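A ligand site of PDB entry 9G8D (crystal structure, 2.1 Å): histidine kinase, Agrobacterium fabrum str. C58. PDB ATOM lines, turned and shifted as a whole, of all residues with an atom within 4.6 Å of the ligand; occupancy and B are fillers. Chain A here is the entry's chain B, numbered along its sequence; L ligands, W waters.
A ring nitrogen (NE2) of His 278 is in hydrogen-bond range of an oxygen (O2) of the ligand, 2.8 Å away.
An oxygen (O4) of the ligand is in hydrogen-bond range of the side-chain hydroxyl of Tyr 165, 2.7 Å away.
SG of Cys 13 is covalently linked to C21 of the ligand, 1.7 Å away.
A nitrogen (N4) of the ligand lies close to the side-chain hydroxyl (OH) of Tyr 251 (3.2 Å).
The side-chain carboxylate of Asp 196 sits at hydrogen-bond distance from a nitrogen (N4) of the ligand (3.0 Å).
An oxygen (O3) of the ligand is in salt-bridge range of the guanidinium group of Arg 211, at 2.9 Å.
O of Asp 196 sits at hydrogen-bond distance from N1 of the ligand, 2.7 Å away.
The side-chain carboxylate (OD1) of Asp 196 is in salt-bridge range of the guanidinium group (NH2) of Arg 456, 2.7 Å away.
The side-chain hydroxyl of Ser 462 lies within hydrogen-bond range of the side-chain hydroxyl of Tyr 251 (2.5 Å).
The backbone carbonyl oxygen (O) of Leu 274 is in hydrogen-bond range of the backbone NH (N) of Tyr 165 (3.0 Å).
The guanidinium group of Arg 456 is in hydrogen-bond range of the side-chain hydroxyl of Ser 195 (3.2 Å).
N of Ile 247 is in hydrogen-bond range of OG of Ser 245 (3.0 Å).
NE2 of Gln 190 sits at hydrogen-bond distance from O of Pro 459 (3.3 Å).
The guanidinium group (NH1) of Arg 211 lies within hydrogen-bond range of the backbone carbonyl oxygen (O) of Arg 242, at 2.9 Å.
The backbone NH (N) of Ser 260 is in hydrogen-bond range of the backbone carbonyl oxygen (O) of Ile 213.
Merely in contact with the ligand: Asp 14 (3.7 Å), Phe 187 (3.7 Å), 9IJ 192 (3.5 Å), Ser 195 (3.8 Å), Ile 197 (3.9 Å), Pro 198 (3.2 Å), Ala 201 (3.98 Å), Tyr 205 (3.2 Å), Ile 213 (3.8 Å), Ser 245 (3.995 Å), Ile 247 (3.6 Å), His 248 (3.3 Å), Met 255 (3.8 Å), Ala 276 (3.8 Å), Arg 456 (3.6 Å), Leu 457 (3.8 Å), Pro 459 (3.7 Å) and Ser 462 (3.5 Å).
Of the 31 residues printed, 24 come within 4 Å of the ligand.
Water W6 lies within hydrogen-bond range of O2 of the ligand (2.5 Å), OG of Ser 260 (2.8 Å) and NE2 of His 248 (2.8 Å).
Water W1 bridges O1 of the ligand (2.6 Å) and N of Ser 245 (2.8 Å).
Water W8 bridges an oxygen (O3) of the ligand and the side-chain hydroxyl of Tyr 205.
Water W5 lies within hydrogen-bond range of O6 of the ligand (2.7 Å), NE2 of Gln 190 (2.8 Å) and O of Pro 459 (3.3 Å).
Water W2 bridges a ring nitrogen (ND1) of His 248 and a nitrogen (N3) of the ligand.
Water W4 lies within hydrogen-bond range of the guanidinium group of Arg 242 (2.8 Å) and an oxygen (O1) of the ligand (2.8 Å).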
ATOM      1  N   LEU A  10     -23.273  18.088   9.802  1.00  0.00           N
ATOM      2  CA  LEU A  10     -22.543  18.449  11.056  1.00  0.00           C
ATOM      3  C   LEU A  10     -21.025  18.298  10.879  1.00  0.00           C
ATOM      4  O   LEU A  10     -20.294  18.874  11.696  1.00  0.00           O
ATOM      5  CB  LEU A  10     -23.065  17.590  12.211  1.00  0.00           C
ATOM      6  CG  LEU A  10     -24.539  17.776  12.557  1.00  0.00           C
ATOM      7  CD1 LEU A  10     -24.893  17.010  13.817  1.00  0.00           C
ATOM      8  CD2 LEU A  10     -24.890  19.252  12.714  1.00  0.00           C
ATOM      9  N   CYS A  13     -20.439  21.842   8.313  1.00  0.00           N
ATOM     10  CA  CYS A  13     -21.218  23.118   8.496  1.00  0.00           C
ATOM     11  C   CYS A  13     -20.298  24.240   9.012  1.00  0.00           C
ATOM     12  O   CYS A  13     -20.620  25.426   8.799  1.00  0.00           O
ATOM     13  CB  CYS A  13     -22.452  22.940   9.385  1.00  0.00           C
ATOM     14  SG  CYS A  13     -22.112  22.462  11.104  1.00  0.00           S
ATOM     15  N   ASP A  14     -19.154  23.887   9.606  1.00  0.00           N
ATOM     16  CA  ASP A  14     -18.110  24.854  10.050  1.00  0.00           C
ATOM     17  C   ASP A  14     -17.510  25.605   8.855  1.00  0.00           C
ATOM     18  O   ASP A  14     -16.885  26.660   9.102  1.00  0.00           O
ATOM     19  CB  ASP A  14     -17.012  24.173  10.869  1.00  0.00           C
ATOM     20  CG  ASP A  14     -16.216  23.126  10.107  1.00  0.00           C
ATOM     21  OD1 ASP A  14     -16.661  22.723   9.004  1.00  0.00           O
ATOM     22  OD2 ASP A  14     -15.170  22.713  10.632  1.00  0.00           O
ATOM     23  N   ILE A  18     -22.177  30.049   3.107  1.00  0.00           N
ATOM     24  CA  ILE A  18     -23.525  30.639   3.392  1.00  0.00           C
ATOM     25  C   ILE A  18     -23.678  31.987   2.676  1.00  0.00           C
ATOM     26  O   ILE A  18     -24.809  32.500   2.643  1.00  0.00           O
ATOM     27  CB  ILE A  18     -23.748  30.745   4.910  1.00  0.00           C
ATOM     28  CG1 ILE A  18     -22.699  31.633   5.585  1.00  0.00           C
ATOM     29  CG2 ILE A  18     -23.801  29.348   5.525  1.00  0.00           C
ATOM     30  CD1 ILE A  18     -23.011  31.967   7.028  1.00  0.00           C
ATOM     31  N   TYR A 165     -27.004  38.468  23.615  1.00  0.00           N
ATOM     32  CA  TYR A 165     -25.811  37.623  23.845  1.00  0.00           C
ATOM     33  C   TYR A 165     -24.609  38.536  24.037  1.00  0.00           C
ATOM     34  O   TYR A 165     -24.505  39.541  23.314  1.00  0.00           O
ATOM     35  CB  TYR A 165     -25.557  36.678  22.673  1.00  0.00           C
ATOM     36  CG  TYR A 165     -26.769  36.000  22.083  1.00  0.00           C
ATOM     37  CD1 TYR A 165     -27.779  35.481  22.889  1.00  0.00           C
ATOM     38  CD2 TYR A 165     -26.896  35.872  20.717  1.00  0.00           C
ATOM     39  CE1 TYR A 165     -28.885  34.855  22.336  1.00  0.00           C
ATOM     40  CE2 TYR A 165     -27.994  35.256  20.144  1.00  0.00           C
ATOM     41  CZ  TYR A 165     -28.993  34.743  20.957  1.00  0.00           C
ATOM     42  OH  TYR A 165     -30.057  34.117  20.372  1.00  0.00           O
ATOM     43  N   PHE A 187     -34.004  31.327  28.566  1.00  0.00           N
ATOM     44  CA  PHE A 187     -32.592  31.043  28.237  1.00  0.00           C
ATOM     45  C   PHE A 187     -31.676  31.987  29.018  1.00  0.00           C
ATOM     46  O   PHE A 187     -30.477  32.024  28.733  1.00  0.00           O
ATOM     47  CB  PHE A 187     -32.349  31.165  26.728  1.00  0.00           C
ATOM     48  CG  PHE A 187     -33.150  30.211  25.872  1.00  0.00           C
ATOM     49  CD1 PHE A 187     -33.121  28.850  26.112  1.00  0.00           C
ATOM     50  CD2 PHE A 187     -33.918  30.675  24.816  1.00  0.00           C
ATOM     51  CE1 PHE A 187     -33.844  27.966  25.320  1.00  0.00           C
ATOM     52  CE2 PHE A 187     -34.647  29.792  24.032  1.00  0.00           C
ATOM     53  CZ  PHE A 187     -34.598  28.445  24.273  1.00  0.00           C
ATOM     54  N   GLN A 190     -27.950  31.266  30.252  1.00  0.00           N
ATOM     55  CA  GLN A 190     -27.464  30.103  29.456  1.00  0.00           C
ATOM     56  C   GLN A 190     -26.256  30.552  28.623  1.00  0.00           C
ATOM     57  O   GLN A 190     -26.114  31.747  28.348  1.00  0.00           O
ATOM     58  CB  GLN A 190     -28.592  29.589  28.565  1.00  0.00           C
ATOM     59  CG  GLN A 190     -28.230  28.356  27.759  1.00  0.00           C
ATOM     60  CD  GLN A 190     -29.463  27.540  27.427  1.00  0.00           C
ATOM     61  OE1 GLN A 190     -30.462  27.581  28.136  1.00  0.00           O
ATOM     62  NE2 GLN A 190     -29.371  26.780  26.358  1.00  0.00           N
ATOM     63  N   9IJ A 192     -23.914  29.230  24.959  1.00  0.00           N
ATOM     64  CA  9IJ A 192     -23.822  28.309  23.811  1.00  0.00           C
ATOM     65  C   9IJ A 192     -22.372  28.241  23.315  1.00  0.00           C
ATOM     66  CB  9IJ A 192     -24.801  28.640  22.662  1.00  0.00           C
ATOM     67  CG  9IJ A 192     -24.855  30.091  22.237  1.00  0.00           C
ATOM     68  CD1 9IJ A 192     -24.036  30.520  21.207  1.00  0.00           C
ATOM     69  CD2 9IJ A 192     -25.755  30.997  22.825  1.00  0.00           C
ATOM     70  CE1 9IJ A 192     -24.066  31.844  20.780  1.00  0.00           C
ATOM     71  CE2 9IJ A 192     -25.785  32.321  22.398  1.00  0.00           C
ATOM     72  CZ  9IJ A 192     -24.946  32.742  21.372  1.00  0.00           C
ATOM     73  C01 9IJ A 192     -26.535  30.617  23.788  1.00  0.00           C
ATOM     74  N01 9IJ A 192     -27.155  30.240  24.698  1.00  0.00           N
ATOM     75  O   9IJ A 192     -21.715  29.507  23.366  1.00  0.00           O
ATOM     76  N   SER A 195     -18.867  27.162  18.419  1.00  0.00           N
ATOM     77  CA  SER A 195     -19.164  26.345  17.196  1.00  0.00           C
ATOM     78  C   SER A 195     -20.623  26.525  16.740  1.00  0.00           C
ATOM     79  O   SER A 195     -20.901  26.223  15.548  1.00  0.00           O
ATOM     80  CB  SER A 195     -18.839  24.907  17.422  1.00  0.00           C
ATOM     81  OG  SER A 195     -19.561  24.400  18.525  1.00  0.00           O
ATOM     82  N   ASP A 196     -21.516  27.020  17.607  1.00  0.00           N
ATOM     83  CA  ASP A 196     -22.946  27.245  17.294  1.00  0.00           C
ATOM     84  C   ASP A 196     -23.077  28.373  16.257  1.00  0.00           C
ATOM     85  O   ASP A 196     -24.097  28.375  15.542  1.00  0.00           O
ATOM     86  CB  ASP A 196     -23.778  27.553  18.541  1.00  0.00           C
ATOM     87  CG  ASP A 196     -24.245  26.303  19.285  1.00  0.00           C
ATOM     88  OD1 ASP A 196     -23.679  25.233  19.047  1.00  0.00           O
ATOM     89  OD2 ASP A 196     -25.170  26.432  20.090  1.00  0.00           O
ATOM     90  N   ILE A 197     -22.119  29.304  16.219  1.00  0.00           N
ATOM     91  CA  ILE A 197     -22.052  30.371  15.178  1.00  0.00           C
ATOM     92  C   ILE A 197     -20.725  30.223  14.433  1.00  0.00           C
ATOM     93  O   ILE A 197     -19.689  30.666  14.944  1.00  0.00           O
ATOM     94  CB  ILE A 197     -22.254  31.783  15.751  1.00  0.00           C
ATOM     95  CG1 ILE A 197     -23.452  31.851  16.710  1.00  0.00           C
ATOM     96  CG2 ILE A 197     -22.386  32.778  14.605  1.00  0.00           C
ATOM     97  CD1 ILE A 197     -23.705  33.213  17.315  1.00  0.00           C
ATOM     98  N   PRO A 198     -20.697  29.615  13.229  1.00  0.00           N
ATOM     99  CA  PRO A 198     -19.449  29.409  12.494  1.00  0.00           C
ATOM    100  C   PRO A 198     -18.868  30.750  12.017  1.00  0.00           C
ATOM    101  O   PRO A 198     -19.589  31.732  12.006  1.00  0.00           O
ATOM    102  CB  PRO A 198     -19.816  28.481  11.321  1.00  0.00           C
ATOM    103  CG  PRO A 198     -21.315  28.620  11.171  1.00  0.00           C
ATOM    104  CD  PRO A 198     -21.854  29.051  12.526  1.00  0.00           C
ATOM    105  N   ALA A 201     -20.492  33.011   9.420  1.00  0.00           N
ATOM    106  CA  ALA A 201     -21.709  33.635  10.018  1.00  0.00           C
ATOM    107  C   ALA A 201     -21.289  34.863  10.857  1.00  0.00           C
ATOM    108  O   ALA A 201     -21.913  35.913  10.722  1.00  0.00           O
ATOM    109  CB  ALA A 201     -22.468  32.623  10.833  1.00  0.00           C
ATOM    110  N   TYR A 205     -22.280  38.747  10.407  1.00  0.00           N
ATOM    111  CA  TYR A 205     -22.849  39.525  11.537  1.00  0.00           C
ATOM    112  C   TYR A 205     -22.035  40.824  11.704  1.00  0.00           C
ATOM    113  O   TYR A 205     -22.629  41.855  12.053  1.00  0.00           O
ATOM    114  CB  TYR A 205     -22.909  38.719  12.839  1.00  0.00           C
ATOM    115  CG  TYR A 205     -23.998  37.677  12.867  1.00  0.00           C
ATOM    116  CD1 TYR A 205     -25.332  38.014  12.639  1.00  0.00           C
ATOM    117  CD2 TYR A 205     -23.713  36.347  13.123  1.00  0.00           C
ATOM    118  CE1 TYR A 205     -26.324  37.055  12.667  1.00  0.00           C
ATOM    119  CE2 TYR A 205     -24.689  35.373  13.140  1.00  0.00           C
ATOM    120  CZ  TYR A 205     -26.009  35.725  12.920  1.00  0.00           C
ATOM    121  OH  TYR A 205     -26.955  34.751  12.935  1.00  0.00           O
ATOM    122  N   ARG A 211     -29.731  40.986  10.412  1.00  0.00           N
ATOM    123  CA  ARG A 211     -29.903  39.661   9.753  1.00  0.00           C
ATOM    124  C   ARG A 211     -31.368  39.253   9.935  1.00  0.00           C
ATOM    125  O   ARG A 211     -31.798  39.101  11.100  1.00  0.00           O
ATOM    126  CB  ARG A 211     -28.911  38.645  10.334  1.00  0.00           C
ATOM    127  CG  ARG A 211     -29.020  37.246   9.722  1.00  0.00           C
ATOM    128  CD  ARG A 211     -29.151  37.247   8.220  1.00  0.00           C
ATOM    129  NE  ARG A 211     -29.096  35.894   7.689  1.00  0.00           N
ATOM    130  CZ  ARG A 211     -29.454  35.531   6.457  1.00  0.00           C
ATOM    131  NH1 ARG A 211     -29.923  36.406   5.588  1.00  0.00           N
ATOM    132  NH2 ARG A 211     -29.345  34.260   6.110  1.00  0.00           N
ATOM    133  N   ILE A 213     -34.587  36.671   9.140  1.00  0.00           N
ATOM    134  CA  ILE A 213     -35.180  35.372   8.711  1.00  0.00           C
ATOM    135  C   ILE A 213     -36.703  35.497   8.863  1.00  0.00           C
ATOM    136  O   ILE A 213     -37.184  35.592  10.017  1.00  0.00           O
ATOM    137  CB  ILE A 213     -34.593  34.194   9.511  1.00  0.00           C
ATOM    138  CG1 ILE A 213     -33.060  34.191   9.452  1.00  0.00           C
ATOM    139  CG2 ILE A 213     -35.184  32.881   9.022  1.00  0.00           C
ATOM    140  CD1 ILE A 213     -32.403  33.086  10.245  1.00  0.00           C
ATOM    141  N   ARG A 242     -30.902  37.152   1.337  1.00  0.00           N
ATOM    142  CA  ARG A 242     -30.080  35.907   1.272  1.00  0.00           C
ATOM    143  C   ARG A 242     -30.721  34.775   2.093  1.00  0.00           C
ATOM    144  O   ARG A 242     -31.070  35.022   3.264  1.00  0.00           O
ATOM    145  CB  ARG A 242     -28.662  36.201   1.757  1.00  0.00           C
ATOM    146  CG  ARG A 242     -27.738  34.990   1.790  1.00  0.00           C
ATOM    147  CD  ARG A 242     -26.329  35.411   2.162  1.00  0.00           C
ATOM    148  NE  ARG A 242     -26.323  36.220   3.376  1.00  0.00           N
ATOM    149  CZ  ARG A 242     -26.154  35.749   4.605  1.00  0.00           C
ATOM    150  NH1 ARG A 242     -26.174  36.595   5.641  1.00  0.00           N
ATOM    151  NH2 ARG A 242     -25.925  34.468   4.823  1.00  0.00           N
ATOM    152  N   VAL A 244     -31.075  31.033   4.167  1.00  0.00           N
ATOM    153  CA  VAL A 244     -30.501  30.624   5.485  1.00  0.00           C
ATOM    154  C   VAL A 244     -29.978  29.199   5.353  1.00  0.00           C
ATOM    155  O   VAL A 244     -30.640  28.406   4.658  1.00  0.00           O
ATOM    156  CB  VAL A 244     -31.550  30.711   6.594  1.00  0.00           C
ATOM    157  CG1 VAL A 244     -30.970  30.326   7.952  1.00  0.00           C
ATOM    158  CG2 VAL A 244     -32.196  32.077   6.639  1.00  0.00           C
ATOM    159  N   SER A 245     -28.852  28.919   6.011  1.00  0.00           N
ATOM    160  CA  SER A 245     -28.295  27.548   6.152  1.00  0.00           C
ATOM    161  C   SER A 245     -29.390  26.586   6.598  1.00  0.00           C
ATOM    162  O   SER A 245     -30.063  26.841   7.593  1.00  0.00           O
ATOM    163  CB  SER A 245     -27.147  27.497   7.100  1.00  0.00           C
ATOM    164  OG  SER A 245     -26.890  26.149   7.477  1.00  0.00           O
ATOM    165  N   ILE A 247     -28.889  24.029   8.277  1.00  0.00           N
ATOM    166  CA  ILE A 247     -28.481  23.640   9.654  1.00  0.00           C
ATOM    167  C   ILE A 247     -29.193  24.555  10.653  1.00  0.00           C
ATOM    168  O   ILE A 247     -29.792  24.043  11.623  1.00  0.00           O
ATOM    169  CB  ILE A 247     -26.955  23.706   9.809  1.00  0.00           C
ATOM    170  CG1 ILE A 247     -26.247  22.626   8.983  1.00  0.00           C
ATOM    171  CG2 ILE A 247     -26.553  23.651  11.274  1.00  0.00           C
ATOM    172  CD1 ILE A 247     -26.629  21.207   9.345  1.00  0.00           C
ATOM    173  N   HIS A 248     -29.124  25.866  10.432  1.00  0.00           N
ATOM    174  CA  HIS A 248     -29.724  26.867  11.367  1.00  0.00           C
ATOM    175  C   HIS A 248     -31.250  26.811  11.299  1.00  0.00           C
ATOM    176  O   HIS A 248     -31.895  26.970  12.355  1.00  0.00           O
ATOM    177  CB  HIS A 248     -29.206  28.280  11.072  1.00  0.00           C
ATOM    178  CG  HIS A 248     -29.699  29.252  12.080  1.00  0.00           C
ATOM    179  ND1 HIS A 248     -29.487  29.071  13.429  1.00  0.00           N
ATOM    180  CD2 HIS A 248     -30.446  30.379  11.953  1.00  0.00           C
ATOM    181  CE1 HIS A 248     -30.051  30.067  14.086  1.00  0.00           C
ATOM    182  NE2 HIS A 248     -30.641  30.880  13.208  1.00  0.00           N
ATOM    183  N   TYR A 251     -32.196  23.961  13.425  1.00  0.00           N
ATOM    184  CA  TYR A 251     -31.999  24.402  14.827  1.00  0.00           C
ATOM    185  C   TYR A 251     -33.231  25.194  15.275  1.00  0.00           C
ATOM    186  O   TYR A 251     -33.829  24.854  16.311  1.00  0.00           O
ATOM    187  CB  TYR A 251     -30.705  25.199  14.992  1.00  0.00           C
ATOM    188  CG  TYR A 251     -30.210  25.235  16.415  1.00  0.00           C
ATOM    189  CD1 TYR A 251     -30.959  25.829  17.418  1.00  0.00           C
ATOM    190  CD2 TYR A 251     -29.001  24.647  16.760  1.00  0.00           C
ATOM    191  CE1 TYR A 251     -30.522  25.850  18.721  1.00  0.00           C
ATOM    192  CE2 TYR A 251     -28.558  24.643  18.072  1.00  0.00           C
ATOM    193  CZ  TYR A 251     -29.328  25.247  19.058  1.00  0.00           C
ATOM    194  OH  TYR A 251     -28.893  25.272  20.347  1.00  0.00           O
ATOM    195  N   MET A 255     -36.391  24.452  18.061  1.00  0.00           N
ATOM    196  CA  MET A 255     -36.735  25.410  19.148  1.00  0.00           C
ATOM    197  C   MET A 255     -38.234  25.752  19.084  1.00  0.00           C
ATOM    198  O   MET A 255     -38.781  26.183  20.101  1.00  0.00           O
ATOM    199  CB  MET A 255     -35.927  26.701  19.019  1.00  0.00           C
ATOM    200  CG  MET A 255     -34.454  26.539  19.319  1.00  0.00           C
ATOM    201  SD  MET A 255     -33.587  28.103  19.083  1.00  0.00           S
ATOM    202  CE  MET A 255     -34.118  28.992  20.532  1.00  0.00           C
ATOM    203  N   SER A 260     -36.708  35.351  12.776  1.00  0.00           N
ATOM    204  CA  SER A 260     -35.746  36.094  13.633  1.00  0.00           C
ATOM    205  C   SER A 260     -35.322  37.401  12.975  1.00  0.00           C
ATOM    206  O   SER A 260     -35.449  37.546  11.735  1.00  0.00           O
ATOM    207  CB  SER A 260     -34.546  35.237  13.996  1.00  0.00           C
ATOM    208  OG  SER A 260     -33.713  34.974  12.872  1.00  0.00           O
ATOM    209  N   LEU A 274     -25.068  40.181  20.049  1.00  0.00           N
ATOM    210  CA  LEU A 274     -26.269  40.387  19.204  1.00  0.00           C
ATOM    211  C   LEU A 274     -27.444  40.758  20.099  1.00  0.00           C
ATOM    212  O   LEU A 274     -27.492  40.284  21.236  1.00  0.00           O
ATOM    213  CB  LEU A 274     -26.613  39.111  18.429  1.00  0.00           C
ATOM    214  CG  LEU A 274     -25.543  38.534  17.520  1.00  0.00           C
ATOM    215  CD1 LEU A 274     -25.983  37.155  17.029  1.00  0.00           C
ATOM    216  CD2 LEU A 274     -25.269  39.467  16.353  1.00  0.00           C
ATOM    217  N   ALA A 276     -30.861  39.566  19.578  1.00  0.00           N
ATOM    218  CA  ALA A 276     -31.519  38.492  18.812  1.00  0.00           C
ATOM    219  C   ALA A 276     -33.013  38.545  19.086  1.00  0.00           C
ATOM    220  O   ALA A 276     -33.409  38.400  20.263  1.00  0.00           O
ATOM    221  CB  ALA A 276     -30.939  37.145  19.172  1.00  0.00           C
ATOM    222  N   HIS A 278     -36.549  36.716  18.296  1.00  0.00           N
ATOM    223  CA  HIS A 278     -37.082  35.397  17.852  1.00  0.00           C
ATOM    224  C   HIS A 278     -38.612  35.447  17.868  1.00  0.00           C
ATOM    225  O   HIS A 278     -39.178  35.942  18.862  1.00  0.00           O
ATOM    226  CB  HIS A 278     -36.557  34.252  18.726  1.00  0.00           C
ATOM    227  CG  HIS A 278     -35.113  33.913  18.543  1.00  0.00           C
ATOM    228  ND1 HIS A 278     -34.473  32.975  19.338  1.00  0.00           N
ATOM    229  CD2 HIS A 278     -34.182  34.363  17.674  1.00  0.00           C
ATOM    230  CE1 HIS A 278     -33.218  32.864  18.965  1.00  0.00           C
ATOM    231  NE2 HIS A 278     -33.006  33.711  17.953  1.00  0.00           N
ATOM    232  N   ARG A 456     -27.982  17.479  18.358  1.00  0.00           N
ATOM    233  CA  ARG A 456     -26.914  18.532  18.312  1.00  0.00           C
ATOM    234  C   ARG A 456     -27.565  19.918  18.159  1.00  0.00           C
ATOM    235  O   ARG A 456     -27.097  20.864  18.809  1.00  0.00           O
ATOM    236  CB  ARG A 456     -25.914  18.295  17.173  1.00  0.00           C
ATOM    237  CG  ARG A 456     -24.901  19.423  16.971  1.00  0.00           C
ATOM    238  CD  ARG A 456     -24.078  19.729  18.216  1.00  0.00           C
ATOM    239  NE  ARG A 456     -23.133  20.845  18.053  1.00  0.00           N
ATOM    240  CZ  ARG A 456     -23.397  22.126  18.291  1.00  0.00           C
ATOM    241  NH1 ARG A 456     -24.602  22.514  18.702  1.00  0.00           N
ATOM    242  NH2 ARG A 456     -22.449  23.036  18.121  1.00  0.00           N
ATOM    243  N   LEU A 457     -28.625  20.010  17.362  1.00  0.00           N
ATOM    244  CA  LEU A 457     -29.241  21.311  16.968  1.00  0.00           C
ATOM    245  C   LEU A 457     -30.385  21.660  17.930  1.00  0.00           C
ATOM    246  O   LEU A 457     -31.493  21.982  17.458  1.00  0.00           O
ATOM    247  CB  LEU A 457     -29.709  21.217  15.511  1.00  0.00           C
ATOM    248  CG  LEU A 457     -28.613  20.905  14.495  1.00  0.00           C
ATOM    249  CD1 LEU A 457     -29.181  20.916  13.086  1.00  0.00           C
ATOM    250  CD2 LEU A 457     -27.455  21.882  14.580  1.00  0.00           C
ATOM    251  N   PRO A 459     -31.053  23.752  22.006  1.00  0.00           N
ATOM    252  CA  PRO A 459     -30.478  24.491  23.137  1.00  0.00           C
ATOM    253  C   PRO A 459     -29.962  23.602  24.273  1.00  0.00           C
ATOM    254  O   PRO A 459     -28.942  23.936  24.838  1.00  0.00           O
ATOM    255  CB  PRO A 459     -31.639  25.396  23.585  1.00  0.00           C
ATOM    256  CG  PRO A 459     -32.449  25.604  22.329  1.00  0.00           C
ATOM    257  CD  PRO A 459     -32.384  24.261  21.627  1.00  0.00           C
ATOM    258  N   SER A 462     -26.598  22.220  23.027  1.00  0.00           N
ATOM    259  CA  SER A 462     -25.681  23.400  22.935  1.00  0.00           C
ATOM    260  C   SER A 462     -25.101  23.689  24.325  1.00  0.00           C
ATOM    261  O   SER A 462     -23.878  23.786  24.444  1.00  0.00           O
ATOM    262  CB  SER A 462     -26.377  24.606  22.365  1.00  0.00           C
ATOM    263  OG  SER A 462     -26.557  24.469  20.972  1.00  0.00           O
HETATM  264  C1  LIG L   1     -25.029  25.129  14.997  1.00  0.00           C
HETATM  265  C2  LIG L   1     -25.235  28.597  12.247  1.00  0.00           C
HETATM  266  O1  LIG L   1     -27.826  32.853   8.224  1.00  0.00           O
HETATM  267  C3  LIG L   1     -27.134  31.005  15.248  1.00  0.00           C
HETATM  268  O2  LIG L   1     -31.101  34.222  16.034  1.00  0.00           O
HETATM  269  C4  LIG L   1     -28.082  28.968  19.461  1.00  0.00           C
HETATM  270  C5  LIG L   1     -24.051  24.510  14.239  1.00  0.00           C
HETATM  271  C6  LIG L   1     -25.307  29.512  11.197  1.00  0.00           C
HETATM  272  O3  LIG L   1     -28.711  34.062   9.850  1.00  0.00           O
HETATM  273  C7  LIG L   1     -27.365  31.959  16.233  1.00  0.00           C
HETATM  274  O4  LIG L   1     -29.653  33.911  17.685  1.00  0.00           O
HETATM  275  C8  LIG L   1     -29.319  29.453  19.884  1.00  0.00           C
HETATM  276  C9  LIG L   1     -23.799  25.173  13.055  1.00  0.00           C
HETATM  277  C10 LIG L   1     -25.977  30.639  11.677  1.00  0.00           C
HETATM  278  C11 LIG L   1     -27.399  31.287  17.434  1.00  0.00           C
HETATM  279  C12 LIG L   1     -29.526  28.961  21.181  1.00  0.00           C
HETATM  280  C13 LIG L   1     -24.562  26.337  13.152  1.00  0.00           C
HETATM  281  C14 LIG L   1     -26.230  30.384  13.019  1.00  0.00           C
HETATM  282  C15 LIG L   1     -27.318  29.911  17.208  1.00  0.00           C
HETATM  283  C16 LIG L   1     -28.432  28.159  21.519  1.00  0.00           C
HETATM  284  C17 LIG L   1     -22.846  24.838  12.046  1.00  0.00           C
HETATM  285  C18 LIG L   1     -26.374  31.870  10.915  1.00  0.00           C
HETATM  286  C19 LIG L   1     -27.504  33.439  16.043  1.00  0.00           C
HETATM  287  C20 LIG L   1     -30.637  29.244  21.999  1.00  0.00           C
HETATM  288  C21 LIG L   1     -21.905  23.845  12.088  1.00  0.00           C
HETATM  289  C22 LIG L   1     -27.825  31.913  10.420  1.00  0.00           C
HETATM  290  C23 LIG L   1     -28.818  33.951  15.462  1.00  0.00           C
HETATM  291  C24 LIG L   1     -30.747  28.987  23.286  1.00  0.00           C
HETATM  292  C25 LIG L   1     -28.140  33.019   9.422  1.00  0.00           C
HETATM  293  C26 LIG L   1     -29.935  34.035  16.468  1.00  0.00           C
HETATM  294  C27 LIG L   1     -24.563  27.380  12.227  1.00  0.00           C
HETATM  295  C28 LIG L   1     -26.949  31.203  13.887  1.00  0.00           C
HETATM  296  C29 LIG L   1     -27.305  29.105  18.325  1.00  0.00           C
HETATM  297  C30 LIG L   1     -23.800  23.035  14.399  1.00  0.00           C
HETATM  298  C31 LIG L   1     -24.821  29.313   9.793  1.00  0.00           C
HETATM  299  C32 LIG L   1     -27.602  31.953  18.762  1.00  0.00           C
HETATM  300  C33 LIG L   1     -30.304  30.271  19.094  1.00  0.00           C
HETATM  301  N1  LIG L   1     -25.323  26.299  14.311  1.00  0.00           N
HETATM  302  O5  LIG L   1     -25.536  24.766  16.030  1.00  0.00           O
HETATM  303  N2  LIG L   1     -25.754  29.153  13.371  1.00  0.00           N
HETATM  304  N3  LIG L   1     -27.001  29.785  15.880  1.00  0.00           N
HETATM  305  N4  LIG L   1     -27.579  28.181  20.458  1.00  0.00           N
HETATM  306  O6  LIG L   1     -28.161  27.560  22.552  1.00  0.00           O
HETATM  307  O   HOH W   1     -26.931  30.883   6.752  1.00  0.00           O
HETATM  308  O   HOH W   2     -27.929  27.343  14.843  1.00  0.00           O
HETATM  309  O   HOH W   3     -22.840  26.796   8.553  1.00  0.00           O
HETATM  310  O   HOH W   4     -25.673  34.606   7.622  1.00  0.00           O
HETATM  311  O   HOH W   5     -27.035  26.638  24.853  1.00  0.00           O
HETATM  312  O   HOH W   6     -31.531  33.517  13.725  1.00  0.00           O
HETATM  313  O   HOH W   7     -31.883  36.677  15.540  1.00  0.00           O
HETATM  314  O   HOH W   8     -29.588  34.990  12.197  1.00  0.00           O
HETATM  315  O   HOH W   9     -19.165  25.276  13.717  1.00  0.00           O
